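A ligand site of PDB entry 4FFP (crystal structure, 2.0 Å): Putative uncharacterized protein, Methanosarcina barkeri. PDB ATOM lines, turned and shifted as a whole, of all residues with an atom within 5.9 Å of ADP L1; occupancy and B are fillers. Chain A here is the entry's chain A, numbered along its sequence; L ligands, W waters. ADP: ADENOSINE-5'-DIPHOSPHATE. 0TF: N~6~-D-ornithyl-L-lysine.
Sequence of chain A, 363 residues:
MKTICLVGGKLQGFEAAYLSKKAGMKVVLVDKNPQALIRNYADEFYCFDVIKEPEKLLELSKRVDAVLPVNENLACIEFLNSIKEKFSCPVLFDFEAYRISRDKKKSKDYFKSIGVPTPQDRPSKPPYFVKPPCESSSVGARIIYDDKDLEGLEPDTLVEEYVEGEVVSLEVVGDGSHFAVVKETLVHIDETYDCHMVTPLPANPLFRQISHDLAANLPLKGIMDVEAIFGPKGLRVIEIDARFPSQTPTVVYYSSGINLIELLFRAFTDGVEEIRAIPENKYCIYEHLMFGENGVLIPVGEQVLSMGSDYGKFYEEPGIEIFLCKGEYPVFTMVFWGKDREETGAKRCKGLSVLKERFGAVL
The backbone NH (N) of Gln 12 sits at hydrogen-bond distance from an oxygen (O10) of 0TF L2, 3.1 Å away.
A nitrogen (N7) of 0TF L2 lies within salt-bridge range of the side-chain carboxylate of Glu 72 (2.8 Å).
The backbone NH (N) of Val 50 is in hydrogen-bond range of a nitrogen (N1) of ADP L1 (3.2 Å).
The side-chain carboxylate (OD1) of Asp 49 is in hydrogen-bond range of a nitrogen (N6) of ADP L1 (2.9 Å).
O3' of ADP L1 lies within hydrogen-bond range of OD2 of Asp 31, 2.6 Å away.
A nitrogen (N7) of ADP L1 lies within hydrogen-bond range of the side-chain amide nitrogen of Asn 73 (2.9 Å).
A nitrogen (N6) of ADP L1 lies within hydrogen-bond range of the side-chain sulfur of Cys 76 (3.7 Å).
An oxygen (O2A) of ADP L1 sits at hydrogen-bond distance from the backbone NH (N) of Glu 72, 2.8 Å away.
The backbone NH (N) of Lys 32 sits at hydrogen-bond distance from a nitrogen (N3) of ADP L1 (3.1 Å).
OE1 of Gln 12 is in hydrogen-bond range of N7 of 0TF L2, at 2.8 Å.
O1B of ADP L1 lies within salt-bridge range of NZ of Lys 10, 3.1 Å away.
O2A of ADP L1 lies within hydrogen-bond range of N7 of 0TF L2.
The backbone NH of Gly 9 sits at hydrogen-bond distance from the side-chain carboxylate of Asp 31.
The side-chain amide nitrogen of Asn 71 sits at hydrogen-bond distance from the backbone carbonyl oxygen of Val 7, 3.2 Å away.
N of Phe 48 lies within hydrogen-bond range of O of Asp 31 (3.2 Å).
NZ of Lys 10 sits close to O of Ser 306.
The backbone NH (N) of Gly 8 is in hydrogen-bond range of the backbone carbonyl oxygen (O) of Val 30 (2.9 Å).
OD1 of Asp 31 sits at hydrogen-bond distance from N of Asn 33, 2.8 Å away.
The backbone NH (N) of Leu 37 lies within hydrogen-bond range of the backbone carbonyl oxygen (O) of Gly 9 (3.2 Å).
The backbone carbonyl oxygen (O) of Phe 48 lies within hydrogen-bond range of the backbone NH (N) of Lys 32, 3.4 Å away.
Residues that only touch ADP L1: Gly 8 (3.2 Å), Gly 9 (3.8 Å), Asn 33 (3.9 Å), Phe 48 (3.5 Å), Ile 51 (3.7 Å) and Asn 71 (3.3 Å).
14 residues have an atom within 4 Å of ADP L1: Gly 8, Gly 9, Lys 10, Asp 31, Lys 32, Asn 33, Phe 48, Asp 49, Val 50, Ile 51, Asn 71, Glu 72, Asn 73 and Cys 76.
Along chain A the residues within 4 Å of ADP L1 span positions 8 to 76.
Water W4 lies within hydrogen-bond range of O9 of 0TF L2 and O1B of ADP L1.
Water W1 lies within hydrogen-bond range of O1A of ADP L1 (2.8 Å) and NZ of Lys 32 (3.4 Å).
Water W3 lies within hydrogen-bond range of the side-chain amide nitrogen (ND2) of Asn 33 (2.7 Å) and an oxygen (O3') of ADP L1 (3.0 Å).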
ATOM      1  N   VAL A   7      -6.187  21.734  10.930  1.00  0.00           N
ATOM      2  CA  VAL A   7      -5.700  22.253  12.223  1.00  0.00           C
ATOM      3  C   VAL A   7      -4.767  21.210  12.871  1.00  0.00           C
ATOM      4  O   VAL A   7      -5.238  20.218  13.456  1.00  0.00           O
ATOM      5  CB  VAL A   7      -6.860  22.651  13.158  1.00  0.00           C
ATOM      6  CG1 VAL A   7      -6.308  23.153  14.496  1.00  0.00           C
ATOM      7  CG2 VAL A   7      -7.800  23.679  12.495  1.00  0.00           C
ATOM      8  N   GLY A   8      -3.467  21.426  12.724  1.00  0.00           N
ATOM      9  CA  GLY A   8      -2.479  20.452  13.154  1.00  0.00           C
ATOM     10  C   GLY A   8      -1.556  20.017  12.035  1.00  0.00           C
ATOM     11  O   GLY A   8      -1.988  19.490  11.003  1.00  0.00           O
ATOM     12  N   GLY A   9      -0.267  20.259  12.235  1.00  0.00           N
ATOM     13  CA  GLY A   9       0.696  20.014  11.164  1.00  0.00           C
ATOM     14  C   GLY A   9       1.791  19.031  11.533  1.00  0.00           C
ATOM     15  O   GLY A   9       2.958  19.242  11.191  1.00  0.00           O
ATOM     16  N   LYS A  10       1.422  17.966  12.239  1.00  0.00           N
ATOM     17  CA  LYS A  10       2.353  16.877  12.484  1.00  0.00           C
ATOM     18  C   LYS A  10       1.984  15.627  11.708  1.00  0.00           C
ATOM     19  O   LYS A  10       1.833  15.714  10.504  1.00  0.00           O
ATOM     20  CB  LYS A  10       2.490  16.601  13.951  1.00  0.00           C
ATOM     21  CG  LYS A  10       3.426  17.590  14.596  1.00  0.00           C
ATOM     22  CD  LYS A  10       3.703  17.227  16.029  1.00  0.00           C
ATOM     23  CE  LYS A  10       4.987  16.445  16.224  1.00  0.00           C
ATOM     24  NZ  LYS A  10       5.236  16.474  17.691  1.00  0.00           N
ATOM     25  N   GLN A  12      -0.661  13.337  11.719  1.00  0.00           N
ATOM     26  CA  GLN A  12      -2.029  13.297  11.192  1.00  0.00           C
ATOM     27  C   GLN A  12      -2.129  14.317  10.076  1.00  0.00           C
ATOM     28  O   GLN A  12      -2.730  14.050   9.058  1.00  0.00           O
ATOM     29  CB  GLN A  12      -3.082  13.653  12.254  1.00  0.00           C
ATOM     30  CG  GLN A  12      -3.341  12.611  13.327  1.00  0.00           C
ATOM     31  CD  GLN A  12      -4.326  13.169  14.317  1.00  0.00           C
ATOM     32  OE1 GLN A  12      -3.947  13.778  15.334  1.00  0.00           O
ATOM     33  NE2 GLN A  12      -5.603  13.126  13.951  1.00  0.00           N
ATOM     34  N   VAL A  30      -3.188  25.327   9.554  1.00  0.00           N
ATOM     35  CA  VAL A  30      -3.052  26.106  10.769  1.00  0.00           C
ATOM     36  C   VAL A  30      -2.320  25.315  11.848  1.00  0.00           C
ATOM     37  O   VAL A  30      -2.711  24.195  12.170  1.00  0.00           O
ATOM     38  CB  VAL A  30      -4.444  26.507  11.312  1.00  0.00           C
ATOM     39  CG1 VAL A  30      -4.330  27.274  12.623  1.00  0.00           C
ATOM     40  CG2 VAL A  30      -5.206  27.319  10.258  1.00  0.00           C
ATOM     41  N   ASP A  31      -1.307  25.920  12.471  1.00  0.00           N
ATOM     42  CA  ASP A  31      -0.597  25.282  13.575  1.00  0.00           C
ATOM     43  C   ASP A  31       0.013  26.385  14.457  1.00  0.00           C
ATOM     44  O   ASP A  31       0.503  27.405  13.956  1.00  0.00           O
ATOM     45  CB  ASP A  31       0.476  24.330  13.040  1.00  0.00           C
ATOM     46  CG  ASP A  31       0.951  23.326  14.071  1.00  0.00           C
ATOM     47  OD1 ASP A  31       1.481  23.735  15.133  1.00  0.00           O
ATOM     48  OD2 ASP A  31       0.816  22.110  13.822  1.00  0.00           O
ATOM     49  N   LYS A  32      -0.022  26.181  15.774  1.00  0.00           N
ATOM     50  CA  LYS A  32       0.514  27.184  16.697  1.00  0.00           C
ATOM     51  C   LYS A  32       2.047  27.117  16.735  1.00  0.00           C
ATOM     52  O   LYS A  32       2.706  28.006  17.276  1.00  0.00           O
ATOM     53  CB  LYS A  32      -0.045  26.978  18.099  1.00  0.00           C
ATOM     54  CG  LYS A  32       0.331  25.621  18.665  1.00  0.00           C
ATOM     55  CD  LYS A  32      -0.231  25.325  20.048  1.00  0.00           C
ATOM     56  CE  LYS A  32       0.129  23.887  20.430  1.00  0.00           C
ATOM     57  NZ  LYS A  32      -0.546  23.466  21.687  1.00  0.00           N
ATOM     58  N   ASN A  33       2.628  26.089  16.141  1.00  0.00           N
ATOM     59  CA  ASN A  33       4.088  25.901  16.195  1.00  0.00           C
ATOM     60  C   ASN A  33       4.741  26.477  14.932  1.00  0.00           C
ATOM     61  O   ASN A  33       4.500  25.968  13.835  1.00  0.00           O
ATOM     62  CB  ASN A  33       4.447  24.401  16.353  1.00  0.00           C
ATOM     63  CG  ASN A  33       5.969  24.105  16.433  1.00  0.00           C
ATOM     64  OD1 ASN A  33       6.811  24.980  16.240  1.00  0.00           O
ATOM     65  ND2 ASN A  33       6.301  22.837  16.683  1.00  0.00           N
ATOM     66  N   ALA A  36       6.184  23.927  12.677  1.00  0.00           N
ATOM     67  CA  ALA A  36       5.259  22.783  12.560  1.00  0.00           C
ATOM     68  C   ALA A  36       5.851  21.894  11.500  1.00  0.00           C
ATOM     69  O   ALA A  36       6.365  22.372  10.505  1.00  0.00           O
ATOM     70  CB  ALA A  36       3.845  23.227  12.172  1.00  0.00           C
ATOM     71  N   LEU A  37       5.816  20.598  11.743  1.00  0.00           N
ATOM     72  CA  LEU A  37       6.501  19.649  10.895  1.00  0.00           C
ATOM     73  C   LEU A  37       6.217  19.751   9.381  1.00  0.00           C
ATOM     74  O   LEU A  37       7.135  19.650   8.540  1.00  0.00           O
ATOM     75  CB  LEU A  37       6.235  18.242  11.472  1.00  0.00           C
ATOM     76  CG  LEU A  37       6.931  17.047  10.869  1.00  0.00           C
ATOM     77  CD1 LEU A  37       8.439  17.144  11.124  1.00  0.00           C
ATOM     78  CD2 LEU A  37       6.347  15.769  11.463  1.00  0.00           C
ATOM     79  N   PHE A  48      -0.890  30.259  14.160  1.00  0.00           N
ATOM     80  CA  PHE A  48      -1.606  30.807  15.298  1.00  0.00           C
ATOM     81  C   PHE A  48      -2.191  29.659  16.085  1.00  0.00           C
ATOM     82  O   PHE A  48      -2.372  28.572  15.554  1.00  0.00           O
ATOM     83  CB  PHE A  48      -2.684  31.860  14.922  1.00  0.00           C
ATOM     84  CG  PHE A  48      -3.861  31.330  14.095  1.00  0.00           C
ATOM     85  CD1 PHE A  48      -3.767  31.231  12.700  1.00  0.00           C
ATOM     86  CD2 PHE A  48      -5.080  30.976  14.714  1.00  0.00           C
ATOM     87  CE1 PHE A  48      -4.850  30.784  11.941  1.00  0.00           C
ATOM     88  CE2 PHE A  48      -6.169  30.502  13.966  1.00  0.00           C
ATOM     89  CZ  PHE A  48      -6.047  30.414  12.576  1.00  0.00           C
ATOM     90  N   ASP A  49      -2.506  29.945  17.337  1.00  0.00           N
ATOM     91  CA  ASP A  49      -3.158  28.994  18.216  1.00  0.00           C
ATOM     92  C   ASP A  49      -4.665  29.267  18.140  1.00  0.00           C
ATOM     93  O   ASP A  49      -5.078  30.377  18.411  1.00  0.00           O
ATOM     94  CB  ASP A  49      -2.656  29.199  19.643  1.00  0.00           C
ATOM     95  CG  ASP A  49      -3.191  28.164  20.575  1.00  0.00           C
ATOM     96  OD1 ASP A  49      -4.384  27.840  20.467  1.00  0.00           O
ATOM     97  OD2 ASP A  49      -2.396  27.600  21.338  1.00  0.00           O
ATOM     98  N   VAL A  50      -5.454  28.279  17.703  1.00  0.00           N
ATOM     99  CA  VAL A  50      -6.845  28.529  17.381  1.00  0.00           C
ATOM    100  C   VAL A  50      -7.635  28.824  18.652  1.00  0.00           C
ATOM    101  O   VAL A  50      -8.651  29.469  18.569  1.00  0.00           O
ATOM    102  CB  VAL A  50      -7.530  27.351  16.629  1.00  0.00           C
ATOM    103  CG1 VAL A  50      -6.794  27.005  15.319  1.00  0.00           C
ATOM    104  CG2 VAL A  50      -7.703  26.159  17.560  1.00  0.00           C
ATOM    105  N   ILE A  51      -7.159  28.355  19.791  1.00  0.00           N
ATOM    106  CA  ILE A  51      -7.801  28.667  21.091  1.00  0.00           C
ATOM    107  C   ILE A  51      -7.539  30.129  21.467  1.00  0.00           C
ATOM    108  O   ILE A  51      -8.377  30.797  22.047  1.00  0.00           O
ATOM    109  CB  ILE A  51      -7.310  27.740  22.244  1.00  0.00           C
ATOM    110  CG1 ILE A  51      -7.486  26.246  21.898  1.00  0.00           C
ATOM    111  CG2 ILE A  51      -8.001  28.043  23.579  1.00  0.00           C
ATOM    112  CD1 ILE A  51      -6.640  25.347  22.794  1.00  0.00           C
ATOM    113  N   VAL A  70      -6.643  17.854  12.961  1.00  0.00           N
ATOM    114  CA  VAL A  70      -5.742  16.725  12.884  1.00  0.00           C
ATOM    115  C   VAL A  70      -4.698  16.898  13.991  1.00  0.00           C
ATOM    116  O   VAL A  70      -3.531  17.121  13.718  1.00  0.00           O
ATOM    117  CB  VAL A  70      -5.087  16.591  11.487  1.00  0.00           C
ATOM    118  CG1 VAL A  70      -5.906  15.695  10.563  1.00  0.00           C
ATOM    119  CG2 VAL A  70      -4.911  17.948  10.819  1.00  0.00           C
ATOM    120  N   ASN A  71      -5.173  16.861  15.229  1.00  0.00           N
ATOM    121  CA  ASN A  71      -4.334  16.897  16.416  1.00  0.00           C
ATOM    122  C   ASN A  71      -5.136  16.215  17.508  1.00  0.00           C
ATOM    123  O   ASN A  71      -6.328  15.996  17.364  1.00  0.00           O
ATOM    124  CB  ASN A  71      -3.964  18.328  16.800  1.00  0.00           C
ATOM    125  CG  ASN A  71      -5.127  19.124  17.374  1.00  0.00           C
ATOM    126  OD1 ASN A  71      -5.442  19.002  18.553  1.00  0.00           O
ATOM    127  ND2 ASN A  71      -5.725  20.006  16.568  1.00  0.00           N
ATOM    128  N   GLU A  72      -4.462  15.876  18.603  1.00  0.00           N
ATOM    129  CA  GLU A  72      -5.066  15.189  19.705  1.00  0.00           C
ATOM    130  C   GLU A  72      -4.834  16.024  20.930  1.00  0.00           C
ATOM    131  O   GLU A  72      -4.689  15.511  22.030  1.00  0.00           O
ATOM    132  CB  GLU A  72      -4.444  13.809  19.852  1.00  0.00           C
ATOM    133  CG  GLU A  72      -4.829  12.932  18.673  1.00  0.00           C
ATOM    134  CD  GLU A  72      -4.076  11.612  18.681  1.00  0.00           C
ATOM    135  OE1 GLU A  72      -2.837  11.638  18.557  1.00  0.00           O
ATOM    136  OE2 GLU A  72      -4.731  10.562  18.798  1.00  0.00           O
ATOM    137  N   ASN A  73      -4.772  17.340  20.742  1.00  0.00           N
ATOM    138  CA  ASN A  73      -4.706  18.229  21.878  1.00  0.00           C
ATOM    139  C   ASN A  73      -6.140  18.363  22.422  1.00  0.00           C
ATOM    140  O   ASN A  73      -6.964  19.047  21.848  1.00  0.00           O
ATOM    141  CB  ASN A  73      -4.077  19.575  21.430  1.00  0.00           C
ATOM    142  CG  ASN A  73      -4.154  20.647  22.489  1.00  0.00           C
ATOM    143  OD1 ASN A  73      -4.538  20.363  23.603  1.00  0.00           O
ATOM    144  ND2 ASN A  73      -3.861  21.891  22.125  1.00  0.00           N
ATOM    145  N   CYS A  76      -7.617  21.769  22.494  1.00  0.00           N
ATOM    146  CA  CYS A  76      -7.963  22.237  21.134  1.00  0.00           C
ATOM    147  C   CYS A  76      -9.323  21.622  20.707  1.00  0.00           C
ATOM    148  O   CYS A  76     -10.255  22.317  20.288  1.00  0.00           O
ATOM    149  CB  CYS A  76      -6.861  21.899  20.088  1.00  0.00           C
ATOM    150  SG  CYS A  76      -7.272  22.570  18.449  1.00  0.00           S
ATOM    151  N   SER A 306       8.119  12.056  14.587  1.00  0.00           N
ATOM    152  CA  SER A 306       7.468  13.219  15.097  1.00  0.00           C
ATOM    153  C   SER A 306       8.420  14.148  15.870  1.00  0.00           C
ATOM    154  O   SER A 306       8.002  15.190  16.382  1.00  0.00           O
ATOM    155  CB  SER A 306       6.329  12.793  16.001  1.00  0.00           C
ATOM    156  OG  SER A 306       6.889  12.585  17.275  1.00  0.00           O
HETATM  157  PB  ADP L   1       2.012  16.198  19.788  1.00  0.00           P
HETATM  158  O1B ADP L   1       2.858  15.117  19.173  1.00  0.00           O
HETATM  159  O2B ADP L   1       1.484  15.792  21.151  1.00  0.00           O
HETATM  160  O3B ADP L   1       2.629  17.588  19.743  1.00  0.00           O
HETATM  161  PA  ADP L   1      -0.675  16.947  19.000  1.00  0.00           P
HETATM  162  O1A ADP L   1      -0.992  17.550  20.352  1.00  0.00           O
HETATM  163  O2A ADP L   1      -1.640  15.988  18.337  1.00  0.00           O
HETATM  164  O3A ADP L   1       0.744  16.227  18.792  1.00  0.00           O
HETATM  165  O5' ADP L   1      -0.562  18.226  18.016  1.00  0.00           O
HETATM  166  C5' ADP L   1      -0.322  18.035  16.623  1.00  0.00           C
HETATM  167  C4' ADP L   1      -0.124  19.390  15.961  1.00  0.00           C
HETATM  168  O4' ADP L   1      -1.312  20.164  16.151  1.00  0.00           O
HETATM  169  C3' ADP L   1       1.052  20.106  16.601  1.00  0.00           C
HETATM  170  O3' ADP L   1       1.932  20.521  15.548  1.00  0.00           O
HETATM  171  C2' ADP L   1       0.386  21.258  17.323  1.00  0.00           C
HETATM  172  O2' ADP L   1       1.307  22.353  17.379  1.00  0.00           O
HETATM  173  C1' ADP L   1      -0.929  21.479  16.550  1.00  0.00           C
HETATM  174  N9  ADP L   1      -1.877  22.026  17.496  1.00  0.00           N
HETATM  175  C8  ADP L   1      -2.259  21.426  18.651  1.00  0.00           C
HETATM  176  N7  ADP L   1      -3.101  22.278  19.308  1.00  0.00           N
HETATM  177  C5  ADP L   1      -3.216  23.402  18.559  1.00  0.00           C
HETATM  178  C6  ADP L   1      -3.961  24.666  18.626  1.00  0.00           C
HETATM  179  N6  ADP L   1      -4.723  25.027  19.662  1.00  0.00           N
HETATM  180  N1  ADP L   1      -3.805  25.518  17.592  1.00  0.00           N
HETATM  181  C2  ADP L   1      -3.042  25.305  16.523  1.00  0.00           C
HETATM  182  N3  ADP L   1      -2.347  24.192  16.386  1.00  0.00           N
HETATM  183  C4  ADP L   1      -2.433  23.225  17.343  1.00  0.00           C
HETATM  184  O18 0TF L   2      -2.753   6.618  13.256  1.00  0.00           O
HETATM  185  C11 0TF L   2      -1.782   6.364  13.965  1.00  0.00           C
HETATM  186  C12 0TF L   2      -1.173   4.961  13.945  1.00  0.00           C
HETATM  187  C14 0TF L   2      -2.091   3.705  13.714  1.00  0.00           C
HETATM  188  C15 0TF L   2      -3.324   4.001  12.834  1.00  0.00           C
HETATM  189  C16 0TF L   2      -3.963   2.739  12.197  1.00  0.00           C
HETATM  190  N17 0TF L   2      -5.134   3.181  11.415  1.00  0.00           N
HETATM  191  N13 0TF L   2      -0.155   5.026  12.876  1.00  0.00           N
HETATM  192  N6  0TF L   2      -1.099   7.289  14.741  1.00  0.00           N
HETATM  193  C5  0TF L   2      -1.540   8.678  15.048  1.00  0.00           C
HETATM  194  C4  0TF L   2      -0.463   9.508  15.812  1.00  0.00           C
HETATM  195  C3  0TF L   2      -0.626  11.063  15.677  1.00  0.00           C
HETATM  196  C2  0TF L   2      -0.045  11.850  16.881  1.00  0.00           C
HETATM  197  C1  0TF L   2      -0.222  13.398  16.805  1.00  0.00           C
HETATM  198  N7  0TF L   2      -1.648  13.701  17.007  1.00  0.00           N
HETATM  199  C8  0TF L   2       0.262  13.963  15.477  1.00  0.00           C
HETATM  200  O10 0TF L   2      -0.610  14.390  14.668  1.00  0.00           O
HETATM  201  O9  0TF L   2       1.503  13.961  15.199  1.00  0.00           O
HETATM  202  O   HOH W   1      -0.409  20.158  21.175  1.00  0.00           O
HETATM  203  O   HOH W   2      -2.879  24.870  22.147  1.00  0.00           O
HETATM  204  O   HOH W   3       4.404  20.951  17.172  1.00  0.00           O
HETATM  205  O   HOH W   4       3.169  13.214  17.150  1.00  0.00           O
